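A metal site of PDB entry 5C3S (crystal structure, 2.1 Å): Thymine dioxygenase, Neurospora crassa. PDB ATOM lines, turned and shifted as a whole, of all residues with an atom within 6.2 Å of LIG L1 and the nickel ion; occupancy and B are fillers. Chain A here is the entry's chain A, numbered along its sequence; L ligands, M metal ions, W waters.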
ATOM      1  N   LYS A 120     -25.806   7.397  14.669  1.00  0.00           N
ATOM      2  CA  LYS A 120     -26.204   8.698  15.174  1.00  0.00           C
ATOM      3  C   LYS A 120     -26.222   9.695  14.035  1.00  0.00           C
ATOM      4  O   LYS A 120     -25.635   9.465  12.984  1.00  0.00           O
ATOM      5  CB  LYS A 120     -25.228   9.188  16.262  1.00  0.00           C
ATOM      6  CG  LYS A 120     -23.831   9.513  15.750  1.00  0.00           C
ATOM      7  CD  LYS A 120     -22.911  10.055  16.845  1.00  0.00           C
ATOM      8  CE  LYS A 120     -21.608  10.592  16.265  1.00  0.00           C
ATOM      9  NZ  LYS A 120     -20.866  11.417  17.250  1.00  0.00           N
ATOM     10  N   ARG A 192     -24.845  21.151  19.912  1.00  0.00           N
ATOM     11  CA  ARG A 192     -24.954  19.932  19.124  1.00  0.00           C
ATOM     12  C   ARG A 192     -26.222  19.157  19.451  1.00  0.00           C
ATOM     13  O   ARG A 192     -26.334  18.548  20.521  1.00  0.00           O
ATOM     14  CB  ARG A 192     -23.732  19.040  19.338  1.00  0.00           C
ATOM     15  CG  ARG A 192     -23.758  17.733  18.554  1.00  0.00           C
ATOM     16  CD  ARG A 192     -22.636  16.804  18.983  1.00  0.00           C
ATOM     17  NE  ARG A 192     -21.513  16.819  18.046  1.00  0.00           N
ATOM     18  CZ  ARG A 192     -20.446  16.021  18.124  1.00  0.00           C
ATOM     19  NH1 ARG A 192     -20.327  15.141  19.115  1.00  0.00           N
ATOM     20  NH2 ARG A 192     -19.492  16.114  17.215  1.00  0.00           N
ATOM     21  N   LEU A 194     -28.397  15.923  18.989  1.00  0.00           N
ATOM     22  CA  LEU A 194     -28.086  14.530  18.674  1.00  0.00           C
ATOM     23  C   LEU A 194     -29.347  13.676  18.610  1.00  0.00           C
ATOM     24  O   LEU A 194     -30.257  13.821  19.427  1.00  0.00           O
ATOM     25  CB  LEU A 194     -27.123  13.934  19.700  1.00  0.00           C
ATOM     26  CG  LEU A 194     -25.666  14.344  19.530  1.00  0.00           C
ATOM     27  CD1 LEU A 194     -24.956  14.378  20.874  1.00  0.00           C
ATOM     28  CD2 LEU A 194     -24.956  13.410  18.568  1.00  0.00           C
ATOM     29  N   TYR A 196     -30.036   9.539  18.050  1.00  0.00           N
ATOM     30  CA  TYR A 196     -29.570   8.176  17.869  1.00  0.00           C
ATOM     31  C   TYR A 196     -30.799   7.366  17.444  1.00  0.00           C
ATOM     32  O   TYR A 196     -31.657   7.102  18.280  1.00  0.00           O
ATOM     33  CB  TYR A 196     -28.989   7.642  19.184  1.00  0.00           C
ATOM     34  CG  TYR A 196     -27.816   8.428  19.732  1.00  0.00           C
ATOM     35  CD1 TYR A 196     -28.018   9.519  20.591  1.00  0.00           C
ATOM     36  CD2 TYR A 196     -26.512   8.097  19.389  1.00  0.00           C
ATOM     37  CE1 TYR A 196     -26.937  10.251  21.091  1.00  0.00           C
ATOM     38  CE2 TYR A 196     -25.432   8.822  19.881  1.00  0.00           C
ATOM     39  CZ  TYR A 196     -25.644   9.887  20.735  1.00  0.00           C
ATOM     40  OH  TYR A 196     -24.561  10.590  21.219  1.00  0.00           O
ATOM     41  N   ALA A 213     -22.087   6.213  20.217  1.00  0.00           N
ATOM     42  CA  ALA A 213     -21.026   7.235  20.083  1.00  0.00           C
ATOM     43  C   ALA A 213     -19.724   6.710  20.654  1.00  0.00           C
ATOM     44  O   ALA A 213     -19.692   6.291  21.803  1.00  0.00           O
ATOM     45  CB  ALA A 213     -21.419   8.524  20.770  1.00  0.00           C
ATOM     46  N   HIS A 216     -14.358   9.084  23.776  1.00  0.00           N
ATOM     47  CA  HIS A 216     -13.675  10.333  23.475  1.00  0.00           C
ATOM     48  C   HIS A 216     -13.621  11.191  24.721  1.00  0.00           C
ATOM     49  O   HIS A 216     -14.265  10.881  25.725  1.00  0.00           O
ATOM     50  CB  HIS A 216     -14.420  11.100  22.383  1.00  0.00           C
ATOM     51  CG  HIS A 216     -15.788  11.550  22.809  1.00  0.00           C
ATOM     52  ND1 HIS A 216     -16.868  10.700  22.845  1.00  0.00           N
ATOM     53  CD2 HIS A 216     -16.248  12.745  23.225  1.00  0.00           C
ATOM     54  CE1 HIS A 216     -17.929  11.346  23.264  1.00  0.00           C
ATOM     55  NE2 HIS A 216     -17.573  12.594  23.514  1.00  0.00           N
ATOM     56  N   THR A 217     -12.848  12.263  24.649  1.00  0.00           N
ATOM     57  CA  THR A 217     -12.914  13.334  25.617  1.00  0.00           C
ATOM     58  C   THR A 217     -13.417  14.555  24.861  1.00  0.00           C
ATOM     59  O   THR A 217     -13.139  14.697  23.663  1.00  0.00           O
ATOM     60  CB  THR A 217     -11.524  13.671  26.219  1.00  0.00           C
ATOM     61  OG1 THR A 217     -10.582  13.903  25.158  1.00  0.00           O
ATOM     62  CG2 THR A 217     -11.011  12.555  27.096  1.00  0.00           C
ATOM     63  N   ASP A 218     -14.171  15.411  25.536  1.00  0.00           N
ATOM     64  CA  ASP A 218     -14.606  16.659  24.950  1.00  0.00           C
ATOM     65  C   ASP A 218     -13.449  17.646  24.930  1.00  0.00           C
ATOM     66  O   ASP A 218     -12.484  17.505  25.698  1.00  0.00           O
ATOM     67  CB  ASP A 218     -15.805  17.243  25.719  1.00  0.00           C
ATOM     68  CG  ASP A 218     -17.056  16.401  25.570  1.00  0.00           C
ATOM     69  OD1 ASP A 218     -17.036  15.431  24.783  1.00  0.00           O
ATOM     70  OD2 ASP A 218     -18.067  16.688  26.246  1.00  0.00           O
ATOM     71  N   THR A 223     -18.954  20.885  29.013  1.00  0.00           N
ATOM     72  CA  THR A 223     -20.036  20.475  28.141  1.00  0.00           C
ATOM     73  C   THR A 223     -21.277  20.305  28.993  1.00  0.00           C
ATOM     74  O   THR A 223     -21.238  19.653  30.051  1.00  0.00           O
ATOM     75  CB  THR A 223     -19.699  19.149  27.438  1.00  0.00           C
ATOM     76  OG1 THR A 223     -18.525  19.319  26.643  1.00  0.00           O
ATOM     77  CG2 THR A 223     -20.846  18.654  26.536  1.00  0.00           C
ATOM     78  N   LEU A 225     -24.599  18.499  29.073  1.00  0.00           N
ATOM     79  CA  LEU A 225     -25.233  17.391  28.394  1.00  0.00           C
ATOM     80  C   LEU A 225     -26.617  17.168  28.954  1.00  0.00           C
ATOM     81  O   LEU A 225     -26.776  16.858  30.135  1.00  0.00           O
ATOM     82  CB  LEU A 225     -24.401  16.099  28.476  1.00  0.00           C
ATOM     83  CG  LEU A 225     -25.080  15.035  27.608  1.00  0.00           C
ATOM     84  CD1 LEU A 225     -24.771  15.230  26.131  1.00  0.00           C
ATOM     85  CD2 LEU A 225     -24.739  13.622  28.027  1.00  0.00           C
ATOM     86  N   PHE A 226     -27.604  17.344  28.089  1.00  0.00           N
ATOM     87  CA  PHE A 226     -28.996  17.098  28.405  1.00  0.00           C
ATOM     88  C   PHE A 226     -29.377  15.783  27.721  1.00  0.00           C
ATOM     89  O   PHE A 226     -29.362  15.682  26.485  1.00  0.00           O
ATOM     90  CB  PHE A 226     -29.877  18.224  27.852  1.00  0.00           C
ATOM     91  CG  PHE A 226     -29.501  19.599  28.344  1.00  0.00           C
ATOM     92  CD1 PHE A 226     -28.522  20.335  27.707  1.00  0.00           C
ATOM     93  CD2 PHE A 226     -30.161  20.160  29.422  1.00  0.00           C
ATOM     94  CE1 PHE A 226     -28.206  21.615  28.126  1.00  0.00           C
ATOM     95  CE2 PHE A 226     -29.828  21.437  29.866  1.00  0.00           C
ATOM     96  CZ  PHE A 226     -28.855  22.161  29.227  1.00  0.00           C
ATOM     97  N   GLN A 227     -29.701  14.760  28.510  1.00  0.00           N
ATOM     98  CA  GLN A 227     -30.091  13.474  27.944  1.00  0.00           C
ATOM     99  C   GLN A 227     -31.551  13.153  28.274  1.00  0.00           C
ATOM    100  O   GLN A 227     -32.077  13.612  29.287  1.00  0.00           O
ATOM    101  CB  GLN A 227     -29.169  12.355  28.412  1.00  0.00           C
ATOM    102  CG  GLN A 227     -29.135  12.125  29.921  1.00  0.00           C
ATOM    103  CD  GLN A 227     -28.270  10.937  30.297  1.00  0.00           C
ATOM    104  OE1 GLN A 227     -28.052  10.032  29.487  1.00  0.00           O
ATOM    105  NE2 GLN A 227     -27.789  10.928  31.527  1.00  0.00           N
ATOM    106  N   LEU A 233     -25.305   6.432  28.056  1.00  0.00           N
ATOM    107  CA  LEU A 233     -24.117   7.244  28.347  1.00  0.00           C
ATOM    108  C   LEU A 233     -23.289   6.526  29.404  1.00  0.00           C
ATOM    109  O   LEU A 233     -23.819   6.106  30.426  1.00  0.00           O
ATOM    110  CB  LEU A 233     -24.486   8.666  28.797  1.00  0.00           C
ATOM    111  CG  LEU A 233     -23.321   9.586  29.224  1.00  0.00           C
ATOM    112  CD1 LEU A 233     -22.425   9.971  28.057  1.00  0.00           C
ATOM    113  CD2 LEU A 233     -23.842  10.834  29.907  1.00  0.00           C
ATOM    114  N   ASN A 255     -19.616  18.032  32.206  1.00  0.00           N
ATOM    115  CA  ASN A 255     -18.235  17.544  32.267  1.00  0.00           C
ATOM    116  C   ASN A 255     -17.199  18.566  31.800  1.00  0.00           C
ATOM    117  O   ASN A 255     -17.456  19.379  30.925  1.00  0.00           O
ATOM    118  CB  ASN A 255     -18.079  16.231  31.502  1.00  0.00           C
ATOM    119  CG  ASN A 255     -18.335  16.367  30.014  1.00  0.00           C
ATOM    120  OD1 ASN A 255     -19.460  16.654  29.608  1.00  0.00           O
ATOM    121  ND2 ASN A 255     -17.314  16.123  29.206  1.00  0.00           N
ATOM    122  N   HIS A 273     -15.679   9.235  27.929  1.00  0.00           N
ATOM    123  CA  HIS A 273     -17.081   8.819  27.973  1.00  0.00           C
ATOM    124  C   HIS A 273     -17.530   8.325  26.597  1.00  0.00           C
ATOM    125  O   HIS A 273     -16.868   8.573  25.597  1.00  0.00           O
ATOM    126  CB  HIS A 273     -17.970   9.951  28.525  1.00  0.00           C
ATOM    127  CG  HIS A 273     -17.825  11.250  27.793  1.00  0.00           C
ATOM    128  ND1 HIS A 273     -16.720  12.060  27.934  1.00  0.00           N
ATOM    129  CD2 HIS A 273     -18.648  11.890  26.941  1.00  0.00           C
ATOM    130  CE1 HIS A 273     -16.855  13.129  27.168  1.00  0.00           C
ATOM    131  NE2 HIS A 273     -18.021  13.052  26.561  1.00  0.00           N
ATOM    132  N   ARG A 274     -18.640   7.600  26.556  1.00  0.00           N
ATOM    133  CA  ARG A 274     -19.145   7.053  25.300  1.00  0.00           C
ATOM    134  C   ARG A 274     -20.641   6.820  25.434  1.00  0.00           C
ATOM    135  O   ARG A 274     -21.182   6.946  26.530  1.00  0.00           O
ATOM    136  CB  ARG A 274     -18.425   5.744  24.948  1.00  0.00           C
ATOM    137  CG  ARG A 274     -18.676   4.630  25.957  1.00  0.00           C
ATOM    138  CD  ARG A 274     -18.033   3.305  25.565  1.00  0.00           C
ATOM    139  NE  ARG A 274     -18.455   2.272  26.498  1.00  0.00           N
ATOM    140  CZ  ARG A 274     -18.023   1.015  26.493  1.00  0.00           C
ATOM    141  NH1 ARG A 274     -17.133   0.607  25.597  1.00  0.00           N
ATOM    142  NH2 ARG A 274     -18.492   0.168  27.395  1.00  0.00           N
ATOM    143  N   VAL A 275     -21.308   6.479  24.334  1.00  0.00           N
ATOM    144  CA  VAL A 275     -22.693   6.025  24.378  1.00  0.00           C
ATOM    145  C   VAL A 275     -22.804   4.645  23.758  1.00  0.00           C
ATOM    146  O   VAL A 275     -22.420   4.437  22.604  1.00  0.00           O
ATOM    147  CB  VAL A 275     -23.670   6.991  23.681  1.00  0.00           C
ATOM    148  CG1 VAL A 275     -25.119   6.546  23.901  1.00  0.00           C
ATOM    149  CG2 VAL A 275     -23.498   8.413  24.188  1.00  0.00           C
ATOM    150  N   ARG A 288     -32.970   7.552  20.743  1.00  0.00           N
ATOM    151  CA  ARG A 288     -32.409   8.300  21.869  1.00  0.00           C
ATOM    152  C   ARG A 288     -32.063   9.736  21.434  1.00  0.00           C
ATOM    153  O   ARG A 288     -31.425   9.939  20.397  1.00  0.00           O
ATOM    154  CB  ARG A 288     -31.166   7.579  22.416  1.00  0.00           C
ATOM    155  CG  ARG A 288     -30.368   8.393  23.428  1.00  0.00           C
ATOM    156  CD  ARG A 288     -29.331   7.563  24.180  1.00  0.00           C
ATOM    157  NE  ARG A 288     -28.797   8.329  25.309  1.00  0.00           N
ATOM    158  CZ  ARG A 288     -27.824   9.240  25.218  1.00  0.00           C
ATOM    159  NH1 ARG A 288     -27.230   9.491  24.051  1.00  0.00           N
ATOM    160  NH2 ARG A 288     -27.419   9.889  26.299  1.00  0.00           N
ATOM    161  N   SER A 290     -30.304  13.415  22.707  1.00  0.00           N
ATOM    162  CA  SER A 290     -29.560  14.212  23.675  1.00  0.00           C
ATOM    163  C   SER A 290     -29.146  15.523  23.012  1.00  0.00           C
ATOM    164  O   SER A 290     -29.256  15.683  21.800  1.00  0.00           O
ATOM    165  CB  SER A 290     -28.337  13.457  24.200  1.00  0.00           C
ATOM    166  OG  SER A 290     -27.412  13.222  23.160  1.00  0.00           O
ATOM    167  N   ILE A 291     -28.696  16.446  23.837  1.00  0.00           N
ATOM    168  CA  ILE A 291     -28.180  17.716  23.354  1.00  0.00           C
ATOM    169  C   ILE A 291     -26.913  18.024  24.128  1.00  0.00           C
ATOM    170  O   ILE A 291     -26.937  18.123  25.354  1.00  0.00           O
ATOM    171  CB  ILE A 291     -29.179  18.876  23.563  1.00  0.00           C
ATOM    172  CG1 ILE A 291     -30.538  18.561  22.905  1.00  0.00           C
ATOM    173  CG2 ILE A 291     -28.608  20.162  22.999  1.00  0.00           C
ATOM    174  CD1 ILE A 291     -31.587  19.619  23.145  1.00  0.00           C
ATOM    175  N   ALA A 292     -25.811  18.152  23.386  1.00  0.00           N
ATOM    176  CA  ALA A 292     -24.527  18.489  23.964  1.00  0.00           C
ATOM    177  C   ALA A 292     -24.213  19.933  23.602  1.00  0.00           C
ATOM    178  O   ALA A 292     -24.034  20.271  22.436  1.00  0.00           O
ATOM    179  CB  ALA A 292     -23.445  17.561  23.437  1.00  0.00           C
ATOM    180  N   PHE A 294     -21.390  22.288  23.843  1.00  0.00           N
ATOM    181  CA  PHE A 294     -19.957  22.399  24.056  1.00  0.00           C
ATOM    182  C   PHE A 294     -19.590  23.850  24.355  1.00  0.00           C
ATOM    183  O   PHE A 294     -19.773  24.727  23.525  1.00  0.00           O
ATOM    184  CB  PHE A 294     -19.201  21.932  22.797  1.00  0.00           C
ATOM    185  CG  PHE A 294     -19.516  20.503  22.387  1.00  0.00           C
ATOM    186  CD1 PHE A 294     -19.294  19.451  23.255  1.00  0.00           C
ATOM    187  CD2 PHE A 294     -20.023  20.229  21.119  1.00  0.00           C
ATOM    188  CE1 PHE A 294     -19.575  18.141  22.878  1.00  0.00           C
ATOM    189  CE2 PHE A 294     -20.299  18.933  20.745  1.00  0.00           C
ATOM    190  CZ  PHE A 294     -20.085  17.890  21.619  1.00  0.00           C
HETATM  191  C1  LIG L   1     -20.766  14.177  22.678  1.00  0.00           C
HETATM  192  O1  LIG L   1     -19.633  14.664  22.878  1.00  0.00           O
HETATM  193  O2  LIG L   1     -21.439  14.507  21.673  1.00  0.00           O
HETATM  194  C2  LIG L   1     -21.294  13.191  23.628  1.00  0.00           C
HETATM  195  O3  LIG L   1     -20.568  12.758  24.527  1.00  0.00           O
HETATM  196  C3  LIG L   1     -22.733  12.719  23.506  1.00  0.00           C
HETATM  197  C4  LIG L   1     -23.190  12.039  24.783  1.00  0.00           C
HETATM  198  C5  LIG L   1     -24.653  11.685  24.702  1.00  0.00           C
HETATM  199  O4  LIG L   1     -25.244  11.368  25.755  1.00  0.00           O
HETATM  200  O5  LIG L   1     -25.235  11.690  23.587  1.00  0.00           O
HETATM  201  N1  LG2 L   2     -17.199  18.862  18.803  1.00  0.00           N
HETATM  202  N2  LG2 L   2     -16.419  19.901  20.835  1.00  0.00           N
HETATM  203  C1  LG2 L   2     -16.269  18.629  21.411  1.00  0.00           C
HETATM  204  C2  LG2 L   2     -16.597  17.506  20.655  1.00  0.00           C
HETATM  205  C3  LG2 L   2     -17.055  17.660  19.341  1.00  0.00           C
HETATM  206  O1  LG2 L   2     -15.858  18.529  22.566  1.00  0.00           O
HETATM  207  C4  LG2 L   2     -16.882  20.018  19.524  1.00  0.00           C
HETATM  208  O2  LG2 L   2     -17.019  21.114  19.000  1.00  0.00           O
HETATM  209  C5  LG2 L   2     -16.465  16.225  21.190  1.00  0.00           C
HETATM  210  O3  LG2 L   2     -17.364  15.386  21.057  1.00  0.00           O
HETATM  211 NI    NI M   1     -18.794  14.064  24.720  1.00  0.00          NI
HETATM  212  O   HOH W   1     -20.077  15.462  25.912  1.00  0.00           O
HETATM  213  O   HOH W   2     -22.023  12.111  20.025  1.00  0.00           O
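The guanidinium group of Arg 288 is in salt-bridge range of an oxygen (O4) of LIG L1, 2.7 Å away. An oxygen (O5) of LIG L1 is in hydrogen-bond range of the side-chain hydroxyl (OH) of Tyr 196 (2.7 Å). OG of Ser 290 is in hydrogen-bond range of O5 of LIG L1 (2.7 Å). NH1 of Arg 192 lies within salt-bridge range of O2 of LIG L1 (2.9 Å).
The side-chain carboxylate of Asp 218 lies within hydrogen-bond range of the side-chain amide nitrogen of Asn 255, at 3.1 Å. The side-chain hydroxyl (OG1) of Thr 223 is in hydrogen-bond range of the side-chain carboxylate (OD2) of Asp 218, 2.7 Å away. O of Arg 288 is in hydrogen-bond range of N of Tyr 196 (2.8 Å). OE1 of Gln 227 sits at hydrogen-bond distance from NH2 of Arg 288, 3.3 Å away. The backbone carbonyl oxygen of Ser 290 is in hydrogen-bond range of the backbone NH of Leu 194, 2.9 Å away. The backbone NH (N) of Arg 192 is in hydrogen-bond range of the backbone carbonyl oxygen (O) of Ala 292, 2.8 Å away. O of Val 275 sits at hydrogen-bond distance from N of Ala 213.
Merely in contact with LIG L1: Leu 194, Leu 225, Leu 233, Val 275 and Phe 294. Hydrophobic or aromatic side chains that line LIG L1: Leu 194, Tyr 196, His 216, Leu 225, Leu 233, His 273, Val 275 and Phe 294. Within 4 Å of LIG L1: Arg 192, Leu 194, Tyr 196, His 216, Asp 218, Leu 225, Leu 233, His 273, Val 275, Arg 288, Ser 290 and Phe 294. The nearest printed residue that does not touch LIG L1 is Ala 292 (4.1 Å).
Three residues have an atom within 4 Å of the nickel ion: His 216, Asp 218 and His 273.
The nickel ion is bound by O1 of LIG L1. O3 of LIG L1 is bound to the nickel ion (2.2 Å). OD1 of Asp 218 binds the nickel ion. The nickel ion is bound by a ring nitrogen (NE2) of His 273, 2.2 Å away. The nickel ion is bound by water W1, 2.2 Å away. The nickel ion is bound by a ring nitrogen (NE2) of His 216 (2.3 Å). The nickel ion has six donor atoms within binding distance.
Water W2 lies within hydrogen-bond range of O2 of LIG L1, NZ of Lys 120 and OH of Tyr 196.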
